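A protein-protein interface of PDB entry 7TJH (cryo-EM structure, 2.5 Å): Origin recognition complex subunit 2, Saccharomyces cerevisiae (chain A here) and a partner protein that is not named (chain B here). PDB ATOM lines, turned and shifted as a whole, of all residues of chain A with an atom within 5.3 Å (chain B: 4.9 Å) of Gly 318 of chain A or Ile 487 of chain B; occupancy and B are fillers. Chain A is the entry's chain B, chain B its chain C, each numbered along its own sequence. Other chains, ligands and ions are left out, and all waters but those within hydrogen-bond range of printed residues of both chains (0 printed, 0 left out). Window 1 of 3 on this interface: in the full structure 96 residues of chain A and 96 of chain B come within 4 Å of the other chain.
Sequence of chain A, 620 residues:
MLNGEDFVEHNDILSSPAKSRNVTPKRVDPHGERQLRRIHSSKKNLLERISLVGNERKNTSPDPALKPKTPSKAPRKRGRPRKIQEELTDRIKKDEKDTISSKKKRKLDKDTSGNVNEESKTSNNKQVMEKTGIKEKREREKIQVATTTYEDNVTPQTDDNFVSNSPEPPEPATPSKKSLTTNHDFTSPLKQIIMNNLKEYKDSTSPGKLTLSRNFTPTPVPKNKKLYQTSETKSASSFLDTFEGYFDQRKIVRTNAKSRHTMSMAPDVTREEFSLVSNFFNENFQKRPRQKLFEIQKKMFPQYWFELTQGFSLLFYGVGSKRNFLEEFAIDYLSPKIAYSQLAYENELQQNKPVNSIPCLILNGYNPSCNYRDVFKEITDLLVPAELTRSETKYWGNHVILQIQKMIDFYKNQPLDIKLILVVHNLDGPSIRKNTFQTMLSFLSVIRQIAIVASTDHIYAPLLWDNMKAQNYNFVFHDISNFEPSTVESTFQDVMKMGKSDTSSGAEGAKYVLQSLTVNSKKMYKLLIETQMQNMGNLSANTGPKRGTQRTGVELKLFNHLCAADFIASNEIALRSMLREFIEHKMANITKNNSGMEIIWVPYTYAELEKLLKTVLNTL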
ATOM      1  N   PHE A 316       4.117 -27.244  26.345  1.00  0.00           N
ATOM      2  CA  PHE A 316       4.070 -25.941  26.978  1.00  0.00           C
ATOM      3  C   PHE A 316       5.381 -25.216  26.722  1.00  0.00           C
ATOM      4  O   PHE A 316       6.457 -25.778  26.932  1.00  0.00           O
ATOM      5  CB  PHE A 316       3.828 -26.087  28.479  1.00  0.00           C
ATOM      6  CG  PHE A 316       2.440 -26.534  28.834  1.00  0.00           C
ATOM      7  CD1 PHE A 316       1.408 -25.615  28.932  1.00  0.00           C
ATOM      8  CD2 PHE A 316       2.170 -27.869  29.092  1.00  0.00           C
ATOM      9  CE1 PHE A 316       0.129 -26.018  29.266  1.00  0.00           C
ATOM     10  CE2 PHE A 316       0.895 -28.279  29.429  1.00  0.00           C
ATOM     11  CZ  PHE A 316      -0.128 -27.353  29.514  1.00  0.00           C
ATOM     12  N   TYR A 317       5.295 -23.978  26.262  1.00  0.00           N
ATOM     13  CA  TYR A 317       6.480 -23.172  26.027  1.00  0.00           C
ATOM     14  C   TYR A 317       6.262 -21.791  26.620  1.00  0.00           C
ATOM     15  O   TYR A 317       5.145 -21.410  26.976  1.00  0.00           O
ATOM     16  CB  TYR A 317       6.814 -23.079  24.531  1.00  0.00           C
ATOM     17  CG  TYR A 317       5.845 -22.249  23.717  1.00  0.00           C
ATOM     18  CD1 TYR A 317       4.615 -22.765  23.325  1.00  0.00           C
ATOM     19  CD2 TYR A 317       6.165 -20.949  23.333  1.00  0.00           C
ATOM     20  CE1 TYR A 317       3.728 -22.011  22.588  1.00  0.00           C
ATOM     21  CE2 TYR A 317       5.284 -20.188  22.598  1.00  0.00           C
ATOM     22  CZ  TYR A 317       4.069 -20.725  22.227  1.00  0.00           C
ATOM     23  OH  TYR A 317       3.191 -19.971  21.492  1.00  0.00           O
ATOM     24  N   GLY A 318       7.340 -21.045  26.736  1.00  0.00           N
ATOM     25  CA  GLY A 318       7.240 -19.677  27.197  1.00  0.00           C
ATOM     26  C   GLY A 318       8.537 -19.209  27.818  1.00  0.00           C
ATOM     27  O   GLY A 318       9.516 -19.941  27.907  1.00  0.00           O
ATOM     28  N   VAL A 319       8.513 -17.954  28.243  1.00  0.00           N
ATOM     29  CA  VAL A 319       9.630 -17.332  28.940  1.00  0.00           C
ATOM     30  C   VAL A 319       9.477 -17.609  30.429  1.00  0.00           C
ATOM     31  O   VAL A 319       8.435 -17.308  31.022  1.00  0.00           O
ATOM     32  CB  VAL A 319       9.675 -15.820  28.659  1.00  0.00           C
ATOM     33  CG1 VAL A 319      10.816 -15.170  29.417  1.00  0.00           C
ATOM     34  CG2 VAL A 319       9.805 -15.565  27.167  1.00  0.00           C
ATOM     35  N   GLY A 320      10.509 -18.187  31.031  1.00  0.00           N
ATOM     36  CA  GLY A 320      10.470 -18.580  32.424  1.00  0.00           C
ATOM     37  C   GLY A 320      10.295 -20.079  32.593  1.00  0.00           C
ATOM     38  O   GLY A 320       9.949 -20.813  31.665  1.00  0.00           O
ATOM     39  N   LYS A 322       8.793 -23.611  33.616  1.00  0.00           N
ATOM     40  CA  LYS A 322       7.490 -24.254  33.632  1.00  0.00           C
ATOM     41  C   LYS A 322       7.492 -25.514  34.488  1.00  0.00           C
ATOM     42  O   LYS A 322       6.685 -26.418  34.258  1.00  0.00           O
ATOM     43  CB  LYS A 322       7.053 -24.560  32.202  1.00  0.00           C
ATOM     44  CG  LYS A 322       7.178 -23.363  31.282  1.00  0.00           C
ATOM     45  CD  LYS A 322       7.035 -23.749  29.828  1.00  0.00           C
ATOM     46  CE  LYS A 322       8.391 -23.881  29.187  1.00  0.00           C
ATOM     47  NZ  LYS A 322       9.295 -22.760  29.543  1.00  0.00           N
ATOM     48  N   THR A 456       9.370 -27.087  26.573  1.00  0.00           N
ATOM     49  CA  THR A 456      10.565 -26.737  25.812  1.00  0.00           C
ATOM     50  C   THR A 456      11.047 -25.355  26.223  1.00  0.00           C
ATOM     51  O   THR A 456      10.255 -24.495  26.607  1.00  0.00           O
ATOM     52  CB  THR A 456      10.331 -26.744  24.285  1.00  0.00           C
ATOM     53  OG1 THR A 456       9.256 -25.857  23.952  1.00  0.00           O
ATOM     54  CG2 THR A 456      10.020 -28.141  23.778  1.00  0.00           C
ATOM     55  N   ASP A 457      12.354 -25.141  26.117  1.00  0.00           N
ATOM     56  CA  ASP A 457      12.973 -23.878  26.494  1.00  0.00           C
ATOM     57  C   ASP A 457      13.724 -23.187  25.366  1.00  0.00           C
ATOM     58  O   ASP A 457      13.820 -21.958  25.382  1.00  0.00           O
ATOM     59  CB  ASP A 457      13.943 -24.092  27.667  1.00  0.00           C
ATOM     60  CG  ASP A 457      13.273 -23.928  29.012  1.00  0.00           C
ATOM     61  OD1 ASP A 457      12.194 -23.302  29.068  1.00  0.00           O
ATOM     62  OD2 ASP A 457      13.822 -24.430  30.014  1.00  0.00           O
ATOM     63  N   ILE A 459      14.641 -21.567  21.731  1.00  0.00           N
ATOM     64  CA  ILE A 459      13.896 -20.841  20.710  1.00  0.00           C
ATOM     65  C   ILE A 459      13.815 -21.616  19.395  1.00  0.00           C
ATOM     66  O   ILE A 459      12.946 -21.332  18.563  1.00  0.00           O
ATOM     67  CB  ILE A 459      14.534 -19.447  20.532  1.00  0.00           C
ATOM     68  CG1 ILE A 459      13.541 -18.447  19.932  1.00  0.00           C
ATOM     69  CG2 ILE A 459      15.818 -19.533  19.728  1.00  0.00           C
ATOM     70  CD1 ILE A 459      13.610 -17.087  20.554  1.00  0.00           C
ATOM     71  N   ASP A 479       1.323 -21.267  25.109  1.00  0.00           N
ATOM     72  CA  ASP A 479       2.274 -20.292  25.631  1.00  0.00           C
ATOM     73  C   ASP A 479       1.886 -19.964  27.069  1.00  0.00           C
ATOM     74  O   ASP A 479       0.835 -19.366  27.314  1.00  0.00           O
ATOM     75  CB  ASP A 479       2.272 -19.044  24.752  1.00  0.00           C
ATOM     76  CG  ASP A 479       3.140 -17.921  25.299  1.00  0.00           C
ATOM     77  OD1 ASP A 479       4.148 -18.195  25.985  1.00  0.00           O
ATOM     78  OD2 ASP A 479       2.809 -16.748  25.032  1.00  0.00           O
ATOM     79  N   ILE A 480       2.731 -20.352  28.020  1.00  0.00           N
ATOM     80  CA  ILE A 480       2.465 -20.120  29.434  1.00  0.00           C
ATOM     81  C   ILE A 480       3.602 -19.316  30.052  1.00  0.00           C
ATOM     82  O   ILE A 480       4.040 -19.617  31.170  1.00  0.00           O
ATOM     83  CB  ILE A 480       2.232 -21.438  30.198  1.00  0.00           C
ATOM     84  CG1 ILE A 480       3.305 -22.474  29.872  1.00  0.00           C
ATOM     85  CG2 ILE A 480       0.857 -21.997  29.888  1.00  0.00           C
ATOM     86  CD1 ILE A 480       3.511 -23.444  30.995  1.00  0.00           C
ATOM     87  N   SER A 481       4.127 -18.347  29.293  1.00  0.00           N
ATOM     88  CA  SER A 481       5.189 -17.454  29.755  1.00  0.00           C
ATOM     89  C   SER A 481       4.817 -16.781  31.067  1.00  0.00           C
ATOM     90  O   SER A 481       3.728 -16.222  31.209  1.00  0.00           O
ATOM     91  CB  SER A 481       5.481 -16.381  28.704  1.00  0.00           C
ATOM     92  OG  SER A 481       5.563 -16.923  27.405  1.00  0.00           O
ATOM     93  N   SER B 482       3.358 -19.167  16.026  1.00  0.00           N
ATOM     94  CA  SER B 482       4.574 -18.415  15.733  1.00  0.00           C
ATOM     95  C   SER B 482       5.437 -18.439  16.991  1.00  0.00           C
ATOM     96  O   SER B 482       5.521 -17.466  17.743  1.00  0.00           O
ATOM     97  CB  SER B 482       4.230 -17.000  15.285  1.00  0.00           C
ATOM     98  OG  SER B 482       4.284 -16.088  16.365  1.00  0.00           O
ATOM     99  N   TYR B 483       6.090 -19.592  17.192  1.00  0.00           N
ATOM    100  CA  TYR B 483       6.744 -19.949  18.452  1.00  0.00           C
ATOM    101  C   TYR B 483       7.858 -18.971  18.810  1.00  0.00           C
ATOM    102  O   TYR B 483       7.855 -18.371  19.895  1.00  0.00           O
ATOM    103  CB  TYR B 483       7.278 -21.385  18.313  1.00  0.00           C
ATOM    104  CG  TYR B 483       8.109 -21.985  19.439  1.00  0.00           C
ATOM    105  CD1 TYR B 483       9.482 -21.735  19.549  1.00  0.00           C
ATOM    106  CD2 TYR B 483       7.537 -22.868  20.342  1.00  0.00           C
ATOM    107  CE1 TYR B 483      10.230 -22.294  20.556  1.00  0.00           C
ATOM    108  CE2 TYR B 483       8.288 -23.444  21.344  1.00  0.00           C
ATOM    109  CZ  TYR B 483       9.629 -23.150  21.451  1.00  0.00           C
ATOM    110  OH  TYR B 483      10.377 -23.716  22.452  1.00  0.00           O
ATOM    111  N   LYS B 484       8.806 -18.784  17.889  1.00  0.00           N
ATOM    112  CA  LYS B 484       9.939 -17.899  18.126  1.00  0.00           C
ATOM    113  C   LYS B 484       9.490 -16.446  18.225  1.00  0.00           C
ATOM    114  O   LYS B 484       9.970 -15.701  19.088  1.00  0.00           O
ATOM    115  CB  LYS B 484      10.973 -18.104  17.019  1.00  0.00           C
ATOM    116  CG  LYS B 484      11.975 -16.993  16.817  1.00  0.00           C
ATOM    117  CD  LYS B 484      12.783 -17.241  15.551  1.00  0.00           C
ATOM    118  CE  LYS B 484      14.100 -16.495  15.579  1.00  0.00           C
ATOM    119  NZ  LYS B 484      13.937 -15.102  15.073  1.00  0.00           N
ATOM    120  N   SER B 485       8.528 -16.049  17.386  1.00  0.00           N
ATOM    121  CA  SER B 485       7.985 -14.697  17.457  1.00  0.00           C
ATOM    122  C   SER B 485       7.202 -14.462  18.742  1.00  0.00           C
ATOM    123  O   SER B 485       7.247 -13.357  19.285  1.00  0.00           O
ATOM    124  CB  SER B 485       7.107 -14.419  16.238  1.00  0.00           C
ATOM    125  OG  SER B 485       7.882 -14.406  15.055  1.00  0.00           O
ATOM    126  N   ASN B 486       6.499 -15.482  19.252  1.00  0.00           N
ATOM    127  CA  ASN B 486       5.817 -15.343  20.538  1.00  0.00           C
ATOM    128  C   ASN B 486       6.811 -15.198  21.683  1.00  0.00           C
ATOM    129  O   ASN B 486       6.584 -14.401  22.601  1.00  0.00           O
ATOM    130  CB  ASN B 486       4.890 -16.534  20.795  1.00  0.00           C
ATOM    131  CG  ASN B 486       3.604 -16.457  19.999  1.00  0.00           C
ATOM    132  OD1 ASN B 486       3.104 -15.373  19.708  1.00  0.00           O
ATOM    133  ND2 ASN B 486       3.059 -17.613  19.642  1.00  0.00           N
ATOM    134  N   ILE B 487       7.922 -15.948  21.634  1.00  0.00           N
ATOM    135  CA  ILE B 487       8.964 -15.828  22.659  1.00  0.00           C
ATOM    136  C   ILE B 487       9.572 -14.426  22.641  1.00  0.00           C
ATOM    137  O   ILE B 487       9.719 -13.780  23.688  1.00  0.00           O
ATOM    138  CB  ILE B 487      10.041 -16.912  22.464  1.00  0.00           C
ATOM    139  CG1 ILE B 487       9.481 -18.311  22.742  1.00  0.00           C
ATOM    140  CG2 ILE B 487      11.232 -16.662  23.376  1.00  0.00           C
ATOM    141  CD1 ILE B 487       9.090 -18.551  24.178  1.00  0.00           C
ATOM    142  N   GLU B 488       9.892 -13.921  21.444  1.00  0.00           N
ATOM    143  CA  GLU B 488      10.497 -12.594  21.325  1.00  0.00           C
ATOM    144  C   GLU B 488       9.519 -11.486  21.703  1.00  0.00           C
ATOM    145  O   GLU B 488       9.920 -10.483  22.304  1.00  0.00           O
ATOM    146  CB  GLU B 488      11.023 -12.385  19.907  1.00  0.00           C
ATOM    147  CG  GLU B 488      12.119 -13.348  19.516  1.00  0.00           C
ATOM    148  CD  GLU B 488      12.187 -13.566  18.017  1.00  0.00           C
ATOM    149  OE1 GLU B 488      11.133 -13.510  17.349  1.00  0.00           O
ATOM    150  OE2 GLU B 488      13.289 -13.818  17.503  1.00  0.00           O
ATOM    151  N   ASP B 489       8.235 -11.650  21.362  1.00  0.00           N
ATOM    152  CA  ASP B 489       7.217 -10.665  21.716  1.00  0.00           C
ATOM    153  C   ASP B 489       7.004 -10.630  23.226  1.00  0.00           C
ATOM    154  O   ASP B 489       6.872  -9.550  23.812  1.00  0.00           O
ATOM    155  CB  ASP B 489       5.920 -11.004  20.965  1.00  0.00           C
ATOM    156  CG  ASP B 489       4.700 -10.186  21.411  1.00  0.00           C
ATOM    157  OD1 ASP B 489       4.827  -9.037  21.891  1.00  0.00           O
ATOM    158  OD2 ASP B 489       3.576 -10.711  21.265  1.00  0.00           O
ATOM    159  N   ASN B 490       6.983 -11.802  23.874  1.00  0.00           N
ATOM    160  CA  ASN B 490       6.828 -11.846  25.324  1.00  0.00           C
ATOM    161  C   ASN B 490       8.058 -11.294  26.032  1.00  0.00           C
ATOM    162  O   ASN B 490       7.936 -10.702  27.108  1.00  0.00           O
ATOM    163  CB  ASN B 490       6.559 -13.278  25.786  1.00  0.00           C
ATOM    164  CG  ASN B 490       5.175 -13.764  25.409  1.00  0.00           C
ATOM    165  OD1 ASN B 490       4.201 -13.014  25.467  1.00  0.00           O
ATOM    166  ND2 ASN B 490       5.079 -15.027  25.022  1.00  0.00           N
ATOM    167  N   LEU B 491       9.244 -11.486  25.450  1.00  0.00           N
ATOM    168  CA  LEU B 491      10.462 -10.925  26.025  1.00  0.00           C
ATOM    169  C   LEU B 491      10.479  -9.407  25.901  1.00  0.00           C
ATOM    170  O   LEU B 491      10.797  -8.697  26.860  1.00  0.00           O
ATOM    171  CB  LEU B 491      11.684 -11.530  25.333  1.00  0.00           C
ATOM    172  CG  LEU B 491      12.222 -12.855  25.864  1.00  0.00           C
ATOM    173  CD1 LEU B 491      13.326 -13.367  24.959  1.00  0.00           C
ATOM    174  CD2 LEU B 491      12.721 -12.706  27.289  1.00  0.00           C
ATOM    175  N   MET B 594      18.298 -20.377  26.652  1.00  0.00           N
ATOM    176  CA  MET B 594      17.223 -20.247  25.672  1.00  0.00           C
ATOM    177  C   MET B 594      17.730 -20.256  24.235  1.00  0.00           C
ATOM    178  O   MET B 594      16.942 -20.506  23.318  1.00  0.00           O
ATOM    179  CB  MET B 594      16.427 -18.968  25.925  1.00  0.00           C
ATOM    180  CG  MET B 594      15.557 -19.014  27.163  1.00  0.00           C
ATOM    181  SD  MET B 594      14.780 -17.428  27.511  1.00  0.00           S
ATOM    182  CE  MET B 594      13.491 -17.429  26.275  1.00  0.00           C
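The backbone NH of Ile 459 of chain A lies within hydrogen-bond range of the backbone carbonyl oxygen of Met 594 of chain B.
ND2 of Asn 490 of chain B is in hydrogen-bond range of OD2 of Asp 479 of chain A, at 2.8 Å.
The side-chain hydroxyl (OG) of Ser 481 of chain A lies within hydrogen-bond range of the side-chain amide nitrogen (ND2) of Asn 490 of chain B, 3.1 Å away.
The side-chain hydroxyl (OH) of Tyr 317 of chain A lies within hydrogen-bond range of the side-chain amide nitrogen (ND2) of Asn 486 of chain B, 3.0 Å away.
OH of Tyr 483 of chain B is in hydrogen-bond range of OG1 of Thr 456 of chain A, at 2.8 Å.
Hydrophobic or aromatic side chains of chain A that line the printed part of chain B: Tyr 317, Val 319 and Ile 459.
Among the printed residues, 14 pairs touch across the chains.
Among the printed residues, no Asp or Glu carboxylate lies within 4 Å of a Lys or Arg side-chain nitrogen of the other chain.
N of Ser 481 of chain A lies within hydrogen-bond range of OD1 of Asp 479 of chain A (3.3 Å).
The backbone NH (N) of Val 319 of chain A sits at hydrogen-bond distance from the side-chain hydroxyl (OG) of Ser 481 of chain A (3.2 Å).
The side-chain amino group (NZ) of Lys 322 of chain A is in hydrogen-bond range of the backbone carbonyl oxygen (O) of Gly 318 of chain A, at 3.3 Å.
NZ of Lys 322 of chain A lies within salt-bridge range of OD1 of Asp 457 of chain A (3.0 Å).
The side-chain amino group (NZ) of Lys 484 of chain B is in salt-bridge range of the side-chain carboxylate (OE2) of Glu 488 of chain B (2.8 Å).
The backbone carbonyl oxygen (O) of Phe 316 of chain A is in hydrogen-bond range of the backbone NH (N) of Thr 456 of chain A, at 3.2 Å.
Among the printed residues, pairs that only touch across the chains: Ile 459 of chain A with Tyr 483 of chain B (3.5 Å), Tyr 317 of chain A with Tyr 483 of chain B (3.5 Å), Ile 459 of chain A with Ile 487 of chain B (3.7 Å), Gly 318 of chain A with Ile 487 of chain B (3.7 Å), Val 319 of chain A with Leu 491 of chain B (3.8 Å), Ile 459 of chain A with Lys 484 of chain B (3.8 Å), Asp 457 of chain A with Met 594 of chain B (3.8 Å), Tyr 317 of chain A with Ile 487 of chain B (3.9 Å) and Val 319 of chain A with Ile 487 of chain B (3.9 Å).
Of the printed residues of chain B, Gly 318 of chain A touches Ile 487 (3.7 Å).
Printed residues of chain B within 4 Å of Asp 457 of chain A: Met 594 (3.8 Å).
Ile 480 of chain A touches none of the printed residues of chain B.
Printed residues of chain A within 4 Å of Lys 484 of chain B: Ile 459 (3.8 Å).
Ser 485 of chain B touches none of the printed residues of chain A.
Of the printed residues of chain A, Asn 486 of chain B touches Tyr 317.
Ile 487 of chain B touches just these residues of chain A: Tyr 317, Gly 318, Val 319 and Ile 459.
Of the printed residues of chain A, Asn 490 of chain B touches Asp 479 and Ser 481.
The nearest printed residue of chain B that does not touch Gly 318 of chain A is Met 594 of chain B (5.0 Å).
The nearest residue of chain A that does not touch Ile 487 of chain B is Ser 481 of chain A (5.1 Å).
The nearest printed residue of chain A that does not touch Leu 491 of chain B is Ile 459 of chain A (5.8 Å).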
